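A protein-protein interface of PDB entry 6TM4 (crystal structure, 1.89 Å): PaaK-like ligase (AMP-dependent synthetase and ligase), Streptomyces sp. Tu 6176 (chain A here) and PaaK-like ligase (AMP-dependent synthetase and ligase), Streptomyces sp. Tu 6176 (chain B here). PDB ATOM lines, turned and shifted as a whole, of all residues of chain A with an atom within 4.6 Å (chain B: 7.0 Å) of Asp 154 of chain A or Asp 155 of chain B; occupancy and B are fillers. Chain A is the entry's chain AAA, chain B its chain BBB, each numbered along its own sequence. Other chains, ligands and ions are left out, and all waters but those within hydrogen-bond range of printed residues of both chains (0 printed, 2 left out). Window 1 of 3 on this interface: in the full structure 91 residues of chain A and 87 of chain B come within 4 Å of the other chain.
Asp 154 of chain A touches just these residues of chain B: Tyr 131 (3.8 Å), Gly 132 (3.4 Å) and Asp 155 (2.6 Å).
Asp 155 of chain B touches three residues of chain A.
Gly 153 of chain A touches just one residue of chain B: Gly 132.
Of the printed residues of chain B, Pro 152 of chain A touches Tyr 131, Gly 132, Leu 133 and His 138.
Of the printed residues of chain A, Arg 157 of chain B touches Ser 157.
Of the printed residues of chain B, Tyr 130 of chain A touches Tyr 131 (3.7 Å), His 138 (3.7 Å), Pro 153 (3.5 Å) and Asp 155 (3.7 Å).
Of the printed residues of chain A, Tyr 131 of chain B touches Tyr 130 (3.7 Å), Pro 152 (3.5 Å) and Asp 154 (3.8 Å).
Thr 129 of chain B touches none of the printed residues of chain A.
The nearest residue of chain B that does not touch Asp 154 of chain A is Pro 130 of chain B (5.1 Å).
The nearest printed residue of chain A that does not touch Asp 155 of chain B is Pro 129 of chain A (5.1 Å).
The nearest printed residue of chain B that does not touch Pro 152 of chain A is Pro 130 of chain B (7.8 Å).
Of the 22 printed residues of chain B, 9 touch a printed residue of chain A.
Printed residues of chain B that touch a printed residue of chain A: Tyr 131, Gly 132, Leu 133, His 138, Pro 153, Asp 155, Arg 157, Ala 160 and Thr 161.
Hydrophobic or aromatic side chains of chain B within 4 Å of the printed part of chain A: Tyr 131, Leu 133, His 138, Pro 153 and Ala 160.
Printed residues of chain A that touch a printed residue of chain B: Tyr 130, Gly 131, Pro 152, Gly 153, Asp 154, Ser 157 and Thr 160.
Among the printed residues, no Asp or Glu carboxylate lies within 4 Å of a Lys or Arg side-chain nitrogen of the other chain.
O of Gly 153 of chain A lies within hydrogen-bond range of OG1 of Thr 160 of chain A (2.6 Å).
The backbone carbonyl oxygen (O) of Val 127 of chain B sits at hydrogen-bond distance from the backbone NH (N) of Asp 155 of chain B (3.1 Å).
OG of Ser 158 of chain B lies close to N of Ala 160 of chain B, 3.1 Å away.
The guanidinium group (NH2) of Arg 127 of chain A lies within hydrogen-bond range of the backbone carbonyl oxygen (O) of Asp 154 of chain A (3.0 Å).
The guanidinium group (NH1) of Arg 128 of chain B is in hydrogen-bond range of the backbone carbonyl oxygen (O) of Asp 155 of chain B (3.1 Å).
A ring nitrogen (NE2) of His 138 of chain B lies within hydrogen-bond range of the backbone carbonyl oxygen of Tyr 131 of chain B (2.7 Å).
The backbone carbonyl oxygen (O) of Pro 152 of chain A lies within hydrogen-bond range of the backbone NH (N) of Leu 133 of chain B.
The backbone NH (N) of Gly 131 of chain A sits at hydrogen-bond distance from the side-chain carboxylate (OD2) of Asp 155 of chain B.
The side-chain carboxylate (OD2) of Asp 154 of chain A sits close to the side-chain carboxylate (OD2) of Asp 155 of chain B, 2.6 Å away.
O of Tyr 131 of chain B sits close to O of Pro 152 of chain A (3.5 Å).
The side-chain carboxylate (OD2) of Asp 154 of chain A sits at hydrogen-bond distance from the backbone NH (N) of Gly 132 of chain B (3.4 Å).
Tyr 130 of chain A touches Tyr 131 of chain B.
His 138 of chain B touches Tyr 130 of chain A.
Pro 153 of chain B touches Tyr 130 of chain A (CB to O, 3.5 Å).
Tyr 130 of chain A touches Asp 155 of chain B.
Gly 132 of chain B touches Pro 152 of chain A (C to O, 3.7 Å).
Pro 152 of chain A touches His 138 of chain B.
O of Gly 153 of chain A touches CA of Gly 132 of chain B (3.97 Å).
CB of Tyr 131 of chain B touches OD2 of Asp 154 of chain A (3.8 Å).
Ser 157 of chain A touches Arg 157 of chain B.
CG of Leu 133 of chain B touches CG2 of Thr 160 of chain A (3.9 Å).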
ATOM      1  N   VAL A 126      12.272 -26.944   9.212  1.00  0.00           N
ATOM      2  CA  VAL A 126      13.379 -26.697  10.175  1.00  0.00           C
ATOM      3  C   VAL A 126      12.895 -25.620  11.137  1.00  0.00           C
ATOM      4  O   VAL A 126      12.790 -24.451  10.704  1.00  0.00           O
ATOM      5  CB  VAL A 126      14.664 -26.300   9.447  1.00  0.00           C
ATOM      6  CG1 VAL A 126      15.751 -25.931  10.422  1.00  0.00           C
ATOM      7  CG2 VAL A 126      15.101 -27.394   8.490  1.00  0.00           C
ATOM      8  N   ARG A 127      12.559 -26.012  12.369  1.00  0.00           N
ATOM      9  CA  ARG A 127      11.924 -25.106  13.367  1.00  0.00           C
ATOM     10  C   ARG A 127      12.867 -24.995  14.566  1.00  0.00           C
ATOM     11  O   ARG A 127      12.449 -25.284  15.681  1.00  0.00           O
ATOM     12  CB  ARG A 127      10.510 -25.597  13.718  1.00  0.00           C
ATOM     13  CG  ARG A 127       9.503 -24.481  13.976  1.00  0.00           C
ATOM     14  CD  ARG A 127       9.952 -23.578  15.100  1.00  0.00           C
ATOM     15  NE  ARG A 127       8.858 -22.836  15.710  1.00  0.00           N
ATOM     16  CZ  ARG A 127       8.413 -21.658  15.302  1.00  0.00           C
ATOM     17  NH1 ARG A 127       7.433 -21.061  15.958  1.00  0.00           N
ATOM     18  NH2 ARG A 127       8.946 -21.083  14.232  1.00  0.00           N
ATOM     19  N   THR A 128      14.112 -24.618  14.299  1.00  0.00           N
ATOM     20  CA  THR A 128      15.151 -24.275  15.292  1.00  0.00           C
ATOM     21  C   THR A 128      15.790 -22.966  14.860  1.00  0.00           C
ATOM     22  O   THR A 128      15.584 -22.547  13.728  1.00  0.00           O
ATOM     23  CB  THR A 128      16.209 -25.375  15.437  1.00  0.00           C
ATOM     24  OG1 THR A 128      16.923 -25.493  14.203  1.00  0.00           O
ATOM     25  CG2 THR A 128      15.601 -26.699  15.818  1.00  0.00           C
ATOM     26  N   PRO A 129      16.537 -22.267  15.737  1.00  0.00           N
ATOM     27  CA  PRO A 129      17.051 -20.958  15.389  1.00  0.00           C
ATOM     28  C   PRO A 129      18.116 -21.031  14.293  1.00  0.00           C
ATOM     29  O   PRO A 129      18.929 -21.960  14.320  1.00  0.00           O
ATOM     30  CB  PRO A 129      17.649 -20.419  16.692  1.00  0.00           C
ATOM     31  CG  PRO A 129      16.943 -21.217  17.771  1.00  0.00           C
ATOM     32  CD  PRO A 129      16.760 -22.589  17.149  1.00  0.00           C
ATOM     33  N   TYR A 130      18.146 -19.996  13.446  1.00  0.00           N
ATOM     34  CA  TYR A 130      19.262 -19.706  12.500  1.00  0.00           C
ATOM     35  C   TYR A 130      20.150 -18.568  13.009  1.00  0.00           C
ATOM     36  O   TYR A 130      21.145 -18.214  12.346  1.00  0.00           O
ATOM     37  CB  TYR A 130      18.673 -19.359  11.139  1.00  0.00           C
ATOM     38  CG  TYR A 130      18.100 -20.517  10.370  1.00  0.00           C
ATOM     39  CD1 TYR A 130      16.873 -21.079  10.708  1.00  0.00           C
ATOM     40  CD2 TYR A 130      18.758 -21.021   9.253  1.00  0.00           C
ATOM     41  CE1 TYR A 130      16.301 -22.113   9.967  1.00  0.00           C
ATOM     42  CE2 TYR A 130      18.198 -22.035   8.499  1.00  0.00           C
ATOM     43  CZ  TYR A 130      16.958 -22.564   8.831  1.00  0.00           C
ATOM     44  OH  TYR A 130      16.444 -23.561   8.062  1.00  0.00           O
ATOM     45  N   GLY A 131      19.789 -17.959  14.144  1.00  0.00           N
ATOM     46  CA  GLY A 131      20.516 -16.803  14.689  1.00  0.00           C
ATOM     47  C   GLY A 131      21.762 -17.241  15.418  1.00  0.00           C
ATOM     48  O   GLY A 131      21.656 -17.674  16.593  1.00  0.00           O
ATOM     49  N   PRO A 152      12.317 -23.280   5.832  1.00  0.00           N
ATOM     50  CA  PRO A 152      13.067 -22.660   6.932  1.00  0.00           C
ATOM     51  C   PRO A 152      12.122 -21.927   7.891  1.00  0.00           C
ATOM     52  O   PRO A 152      11.808 -20.776   7.679  1.00  0.00           O
ATOM     53  CB  PRO A 152      14.047 -21.732   6.179  1.00  0.00           C
ATOM     54  CG  PRO A 152      13.254 -21.303   4.974  1.00  0.00           C
ATOM     55  CD  PRO A 152      12.470 -22.532   4.583  1.00  0.00           C
ATOM     56  N   GLY A 153      11.630 -22.635   8.905  1.00  0.00           N
ATOM     57  CA  GLY A 153      10.714 -22.086   9.927  1.00  0.00           C
ATOM     58  C   GLY A 153      11.434 -21.112  10.840  1.00  0.00           C
ATOM     59  O   GLY A 153      10.813 -20.111  11.280  1.00  0.00           O
ATOM     60  N   ASP A 154      12.706 -21.394  11.133  1.00  0.00           N
ATOM     61  CA  ASP A 154      13.485 -20.634  12.131  1.00  0.00           C
ATOM     62  C   ASP A 154      12.737 -20.877  13.457  1.00  0.00           C
ATOM     63  O   ASP A 154      11.793 -21.645  13.467  1.00  0.00           O
ATOM     64  CB  ASP A 154      13.619 -19.183  11.651  1.00  0.00           C
ATOM     65  CG  ASP A 154      14.780 -18.383  12.180  1.00  0.00           C
ATOM     66  OD1 ASP A 154      15.452 -18.888  13.132  1.00  0.00           O
ATOM     67  OD2 ASP A 154      14.956 -17.202  11.680  1.00  0.00           O
ATOM     68  N   ALA A 155      13.185 -20.310  14.546  1.00  0.00           N
ATOM     69  CA  ALA A 155      12.557 -20.423  15.884  1.00  0.00           C
ATOM     70  C   ALA A 155      13.026 -19.202  16.635  1.00  0.00           C
ATOM     71  O   ALA A 155      14.158 -18.728  16.334  1.00  0.00           O
ATOM     72  CB  ALA A 155      12.929 -21.684  16.635  1.00  0.00           C
ATOM     73  N   SER A 157      11.796 -16.359  16.236  1.00  0.00           N
ATOM     74  CA  SER A 157      11.743 -15.247  15.267  1.00  0.00           C
ATOM     75  C   SER A 157      10.330 -14.693  15.270  1.00  0.00           C
ATOM     76  O   SER A 157       9.410 -15.499  15.161  1.00  0.00           O
ATOM     77  CB  SER A 157      12.173 -15.696  13.878  1.00  0.00           C
ATOM     78  OG  SER A 157      11.883 -14.683  12.957  1.00  0.00           O
ATOM     79  N   THR A 160       8.012 -15.918  12.317  1.00  0.00           N
ATOM     80  CA  THR A 160       7.440 -17.281  12.207  1.00  0.00           C
ATOM     81  C   THR A 160       6.805 -17.728  13.525  1.00  0.00           C
ATOM     82  O   THR A 160       7.290 -18.632  14.196  1.00  0.00           O
ATOM     83  CB  THR A 160       8.514 -18.243  11.683  1.00  0.00           C
ATOM     84  OG1 THR A 160       9.685 -18.096  12.487  1.00  0.00           O
ATOM     85  CG2 THR A 160       8.847 -17.965  10.231  1.00  0.00           C
ATOM     86  N   LEU B 126      28.377 -10.481   7.678  1.00  0.00           N
ATOM     87  CA  LEU B 126      27.253 -10.583   8.649  1.00  0.00           C
ATOM     88  C   LEU B 126      25.935 -10.478   7.887  1.00  0.00           C
ATOM     89  O   LEU B 126      25.638  -9.414   7.320  1.00  0.00           O
ATOM     90  CB  LEU B 126      27.368  -9.470   9.693  1.00  0.00           C
ATOM     91  CG  LEU B 126      26.206  -9.371  10.673  1.00  0.00           C
ATOM     92  CD1 LEU B 126      26.139 -10.618  11.534  1.00  0.00           C
ATOM     93  CD2 LEU B 126      26.336  -8.121  11.526  1.00  0.00           C
ATOM     94  N   VAL B 127      25.156 -11.547   7.890  1.00  0.00           N
ATOM     95  CA  VAL B 127      23.818 -11.559   7.234  1.00  0.00           C
ATOM     96  C   VAL B 127      22.788 -11.220   8.312  1.00  0.00           C
ATOM     97  O   VAL B 127      22.572 -12.071   9.222  1.00  0.00           O
ATOM     98  CB  VAL B 127      23.554 -12.926   6.602  1.00  0.00           C
ATOM     99  CG1 VAL B 127      22.140 -13.021   6.062  1.00  0.00           C
ATOM    100  CG2 VAL B 127      24.584 -13.219   5.533  1.00  0.00           C
ATOM    101  N   ARG B 128      22.203 -10.038   8.225  1.00  0.00           N
ATOM    102  CA  ARG B 128      21.348  -9.447   9.283  1.00  0.00           C
ATOM    103  C   ARG B 128      19.985  -9.167   8.650  1.00  0.00           C
ATOM    104  O   ARG B 128      19.507  -8.025   8.722  1.00  0.00           O
ATOM    105  CB  ARG B 128      22.041  -8.228   9.907  1.00  0.00           C
ATOM    106  CG  ARG B 128      21.774  -8.035  11.398  1.00  0.00           C
ATOM    107  CD  ARG B 128      20.334  -8.137  11.760  1.00  0.00           C
ATOM    108  NE  ARG B 128      20.018  -7.504  13.024  1.00  0.00           N
ATOM    109  CZ  ARG B 128      19.898  -8.110  14.175  1.00  0.00           C
ATOM    110  NH1 ARG B 128      20.108  -9.404  14.285  1.00  0.00           N
ATOM    111  NH2 ARG B 128      19.563  -7.398  15.233  1.00  0.00           N
ATOM    112  N   THR B 129      19.398 -10.191   8.022  1.00  0.00           N
ATOM    113  CA  THR B 129      18.008 -10.207   7.533  1.00  0.00           C
ATOM    114  C   THR B 129      17.396 -11.502   8.026  1.00  0.00           C
ATOM    115  O   THR B 129      18.123 -12.388   8.470  1.00  0.00           O
ATOM    116  CB  THR B 129      17.908 -10.071   6.008  1.00  0.00           C
ATOM    117  OG1 THR B 129      18.509 -11.222   5.398  1.00  0.00           O
ATOM    118  CG2 THR B 129      18.587  -8.821   5.497  1.00  0.00           C
ATOM    119  N   PRO B 130      16.057 -11.650   7.985  1.00  0.00           N
ATOM    120  CA  PRO B 130      15.432 -12.842   8.529  1.00  0.00           C
ATOM    121  C   PRO B 130      15.744 -14.095   7.703  1.00  0.00           C
ATOM    122  O   PRO B 130      15.860 -13.996   6.493  1.00  0.00           O
ATOM    123  CB  PRO B 130      13.929 -12.521   8.502  1.00  0.00           C
ATOM    124  CG  PRO B 130      13.879 -11.011   8.420  1.00  0.00           C
ATOM    125  CD  PRO B 130      15.067 -10.646   7.571  1.00  0.00           C
ATOM    126  N   TYR B 131      15.820 -15.234   8.399  1.00  0.00           N
ATOM    127  CA  TYR B 131      15.857 -16.598   7.800  1.00  0.00           C
ATOM    128  C   TYR B 131      14.494 -17.299   7.938  1.00  0.00           C
ATOM    129  O   TYR B 131      14.317 -18.411   7.426  1.00  0.00           O
ATOM    130  CB  TYR B 131      16.942 -17.419   8.491  1.00  0.00           C
ATOM    131  CG  TYR B 131      18.365 -17.062   8.134  1.00  0.00           C
ATOM    132  CD1 TYR B 131      18.958 -15.893   8.590  1.00  0.00           C
ATOM    133  CD2 TYR B 131      19.136 -17.911   7.352  1.00  0.00           C
ATOM    134  CE1 TYR B 131      20.279 -15.583   8.292  1.00  0.00           C
ATOM    135  CE2 TYR B 131      20.456 -17.625   7.049  1.00  0.00           C
ATOM    136  CZ  TYR B 131      21.037 -16.465   7.538  1.00  0.00           C
ATOM    137  OH  TYR B 131      22.340 -16.186   7.239  1.00  0.00           O
ATOM    138  N   GLY B 132      13.540 -16.686   8.637  1.00  0.00           N
ATOM    139  CA  GLY B 132      12.216 -17.284   8.876  1.00  0.00           C
ATOM    140  C   GLY B 132      11.344 -17.135   7.640  1.00  0.00           C
ATOM    141  O   GLY B 132      10.767 -15.996   7.428  1.00  0.00           O
ATOM    142  N   LEU B 133      11.276 -18.196   6.822  1.00  0.00           N
ATOM    143  CA  LEU B 133      10.405 -18.345   5.622  1.00  0.00           C
ATOM    144  C   LEU B 133      10.838 -17.447   4.470  1.00  0.00           C
ATOM    145  O   LEU B 133      10.844 -17.954   3.325  1.00  0.00           O
ATOM    146  CB  LEU B 133       8.924 -18.105   5.934  1.00  0.00           C
ATOM    147  CG  LEU B 133       8.211 -19.247   6.654  1.00  0.00           C
ATOM    148  CD1 LEU B 133       6.730 -18.957   6.832  1.00  0.00           C
ATOM    149  CD2 LEU B 133       8.362 -20.529   5.892  1.00  0.00           C
ATOM    150  N   GLY B 137      17.715 -13.915   4.119  1.00  0.00           N
ATOM    151  CA  GLY B 137      18.890 -14.448   4.840  1.00  0.00           C
ATOM    152  C   GLY B 137      19.542 -15.576   4.062  1.00  0.00           C
ATOM    153  O   GLY B 137      20.799 -15.616   3.949  1.00  0.00           O
ATOM    154  N   HIS B 138      18.720 -16.475   3.537  1.00  0.00           N
ATOM    155  CA  HIS B 138      19.174 -17.651   2.754  1.00  0.00           C
ATOM    156  C   HIS B 138      19.930 -17.170   1.516  1.00  0.00           C
ATOM    157  O   HIS B 138      20.923 -17.809   1.144  1.00  0.00           O
ATOM    158  CB  HIS B 138      17.978 -18.552   2.422  1.00  0.00           C
ATOM    159  CG  HIS B 138      17.283 -19.030   3.654  1.00  0.00           C
ATOM    160  ND1 HIS B 138      17.808 -20.046   4.449  1.00  0.00           N
ATOM    161  CD2 HIS B 138      16.198 -18.528   4.293  1.00  0.00           C
ATOM    162  CE1 HIS B 138      17.007 -20.210   5.498  1.00  0.00           C
ATOM    163  NE2 HIS B 138      16.008 -19.261   5.434  1.00  0.00           N
ATOM    164  N   VAL B 152      28.514 -15.052   8.761  1.00  0.00           N
ATOM    165  CA  VAL B 152      28.014 -14.935  10.158  1.00  0.00           C
ATOM    166  C   VAL B 152      26.503 -14.773  10.062  1.00  0.00           C
ATOM    167  O   VAL B 152      26.032 -13.735   9.610  1.00  0.00           O
ATOM    168  CB  VAL B 152      28.661 -13.765  10.900  1.00  0.00           C
ATOM    169  CG1 VAL B 152      28.200 -13.759  12.354  1.00  0.00           C
ATOM    170  CG2 VAL B 152      30.185 -13.822  10.821  1.00  0.00           C
ATOM    171  N   PRO B 153      25.716 -15.814  10.424  1.00  0.00           N
ATOM    172  CA  PRO B 153      24.259 -15.753  10.330  1.00  0.00           C
ATOM    173  C   PRO B 153      23.667 -14.974  11.514  1.00  0.00           C
ATOM    174  O   PRO B 153      23.443 -15.526  12.567  1.00  0.00           O
ATOM    175  CB  PRO B 153      23.859 -17.234  10.296  1.00  0.00           C
ATOM    176  CG  PRO B 153      24.941 -17.912  11.119  1.00  0.00           C
ATOM    177  CD  PRO B 153      26.201 -17.128  10.863  1.00  0.00           C
ATOM    178  N   GLY B 154      23.466 -13.685  11.315  1.00  0.00           N
ATOM    179  CA  GLY B 154      22.943 -12.808  12.377  1.00  0.00           C
ATOM    180  C   GLY B 154      21.445 -12.981  12.482  1.00  0.00           C
ATOM    181  O   GLY B 154      20.908 -12.711  13.549  1.00  0.00           O
ATOM    182  N   ASP B 155      20.776 -13.373  11.397  1.00  0.00           N
ATOM    183  CA  ASP B 155      19.300 -13.467  11.344  1.00  0.00           C
ATOM    184  C   ASP B 155      18.822 -12.044  11.695  1.00  0.00           C
ATOM    185  O   ASP B 155      19.663 -11.136  11.805  1.00  0.00           O
ATOM    186  CB  ASP B 155      18.857 -14.628  12.225  1.00  0.00           C
ATOM    187  CG  ASP B 155      17.493 -15.235  11.947  1.00  0.00           C
ATOM    188  OD1 ASP B 155      16.745 -14.652  11.117  1.00  0.00           O
ATOM    189  OD2 ASP B 155      17.160 -16.297  12.605  1.00  0.00           O
ATOM    190  N   ALA B 156      17.540 -11.807  11.740  1.00  0.00           N
ATOM    191  CA  ALA B 156      16.944 -10.514  12.120  1.00  0.00           C
ATOM    192  C   ALA B 156      15.585 -10.911  12.660  1.00  0.00           C
ATOM    193  O   ALA B 156      15.011 -11.903  12.124  1.00  0.00           O
ATOM    194  CB  ALA B 156      16.865  -9.534  10.959  1.00  0.00           C
ATOM    195  N   ARG B 157      15.146 -10.207  13.694  1.00  0.00           N
ATOM    196  CA  ARG B 157      13.831 -10.397  14.339  1.00  0.00           C
ATOM    197  C   ARG B 157      13.873 -11.663  15.170  1.00  0.00           C
ATOM    198  O   ARG B 157      12.820 -12.133  15.551  1.00  0.00           O
ATOM    199  CB  ARG B 157      12.736 -10.487  13.286  1.00  0.00           C
ATOM    200  CG  ARG B 157      12.872  -9.427  12.208  1.00  0.00           C
ATOM    201  CD  ARG B 157      11.622  -9.436  11.377  1.00  0.00           C
ATOM    202  NE  ARG B 157      11.790  -8.583  10.231  1.00  0.00           N
ATOM    203  CZ  ARG B 157      10.833  -7.859   9.670  1.00  0.00           C
ATOM    204  NH1 ARG B 157       9.602  -7.848  10.155  1.00  0.00           N
ATOM    205  NH2 ARG B 157      11.136  -7.133   8.616  1.00  0.00           N
ATOM    206  N   SER B 158      15.068 -12.142  15.475  1.00  0.00           N
ATOM    207  CA  SER B 158      15.296 -13.315  16.336  1.00  0.00           C
ATOM    208  C   SER B 158      15.680 -12.818  17.736  1.00  0.00           C
ATOM    209  O   SER B 158      16.518 -11.940  17.859  1.00  0.00           O
ATOM    210  CB  SER B 158      16.339 -14.209  15.757  1.00  0.00           C
ATOM    211  OG  SER B 158      16.668 -15.218  16.696  1.00  0.00           O
ATOM    212  N   ALA B 160      17.467 -14.462  19.620  1.00  0.00           N
ATOM    213  CA  ALA B 160      18.877 -14.912  19.739  1.00  0.00           C
ATOM    214  C   ALA B 160      19.860 -13.797  19.372  1.00  0.00           C
ATOM    215  O   ALA B 160      20.984 -13.870  19.853  1.00  0.00           O
ATOM    216  CB  ALA B 160      19.113 -16.128  18.855  1.00  0.00           C
ATOM    217  N   THR B 161      19.484 -12.826  18.524  1.00  0.00           N
ATOM    218  CA  THR B 161      20.450 -11.847  17.961  1.00  0.00           C
ATOM    219  C   THR B 161      19.969 -10.408  18.147  1.00  0.00           C
ATOM    220  O   THR B 161      19.693  -9.705  17.181  1.00  0.00           O
ATOM    221  CB  THR B 161      20.785 -12.203  16.510  1.00  0.00           C
ATOM    222  OG1 THR B 161      19.574 -12.251  15.763  1.00  0.00           O
ATOM    223  CG2 THR B 161      21.490 -13.530  16.406  1.00  0.00           C
ATOM    224  N   MET B 166      25.014  -8.044  17.920  1.00  0.00           N
ATOM    225  CA  MET B 166      25.481  -7.769  16.541  1.00  0.00           C
ATOM    226  C   MET B 166      26.625  -6.745  16.581  1.00  0.00           C
ATOM    227  O   MET B 166      27.605  -6.901  15.816  1.00  0.00           O
ATOM    228  CB  MET B 166      24.335  -7.255  15.669  1.00  0.00           C
ATOM    229  CG  MET B 166      23.223  -8.261  15.508  1.00  0.00           C
ATOM    230  SD  MET B 166      23.738  -9.794  14.673  1.00  0.00           S
ATOM    231  CE  MET B 166      24.204 -10.783  16.094  1.00  0.00           C
ATOM    232  N   TRP B 179      24.673  -7.220   5.419  1.00  0.00           N
ATOM    233  CA  TRP B 179      23.431  -7.246   4.606  1.00  0.00           C
ATOM    234  C   TRP B 179      22.281  -7.034   5.573  1.00  0.00           C
ATOM    235  O   TRP B 179      22.106  -7.863   6.488  1.00  0.00           O
ATOM    236  CB  TRP B 179      23.337  -8.568   3.855  1.00  0.00           C
ATOM    237  CG  TRP B 179      22.020  -8.961   3.261  1.00  0.00           C
ATOM    238  CD1 TRP B 179      21.305 -10.078   3.578  1.00  0.00           C
ATOM    239  CD2 TRP B 179      21.306  -8.330   2.188  1.00  0.00           C
ATOM    240  NE1 TRP B 179      20.188 -10.178   2.790  1.00  0.00           N
ATOM    241  CE2 TRP B 179      20.170  -9.129   1.917  1.00  0.00           C
ATOM    242  CE3 TRP B 179      21.502  -7.165   1.447  1.00  0.00           C
ATOM    243  CZ2 TRP B 179      19.224  -8.787   0.964  1.00  0.00           C
ATOM    244  CZ3 TRP B 179      20.587  -6.856   0.470  1.00  0.00           C
ATOM    245  CH2 TRP B 179      19.467  -7.649   0.238  1.00  0.00           C
ATOM    246  N   GLU B 184      17.821  -0.890   9.550  1.00  0.00           N
ATOM    247  CA  GLU B 184      18.730  -1.705  10.397  1.00  0.00           C
ATOM    248  C   GLU B 184      20.136  -1.098  10.391  1.00  0.00           C
ATOM    249  O   GLU B 184      20.874  -1.228  11.395  1.00  0.00           O
ATOM    250  CB  GLU B 184      18.685  -3.161   9.923  1.00  0.00           C
ATOM    251  CG  GLU B 184      19.291  -4.140  10.888  1.00  0.00           C
ATOM    252  CD  GLU B 184      18.552  -4.329  12.209  1.00  0.00           C
ATOM    253  OE1 GLU B 184      17.363  -3.891  12.322  1.00  0.00           O
ATOM    254  OE2 GLU B 184      19.191  -4.893  13.126  1.00  0.00           O
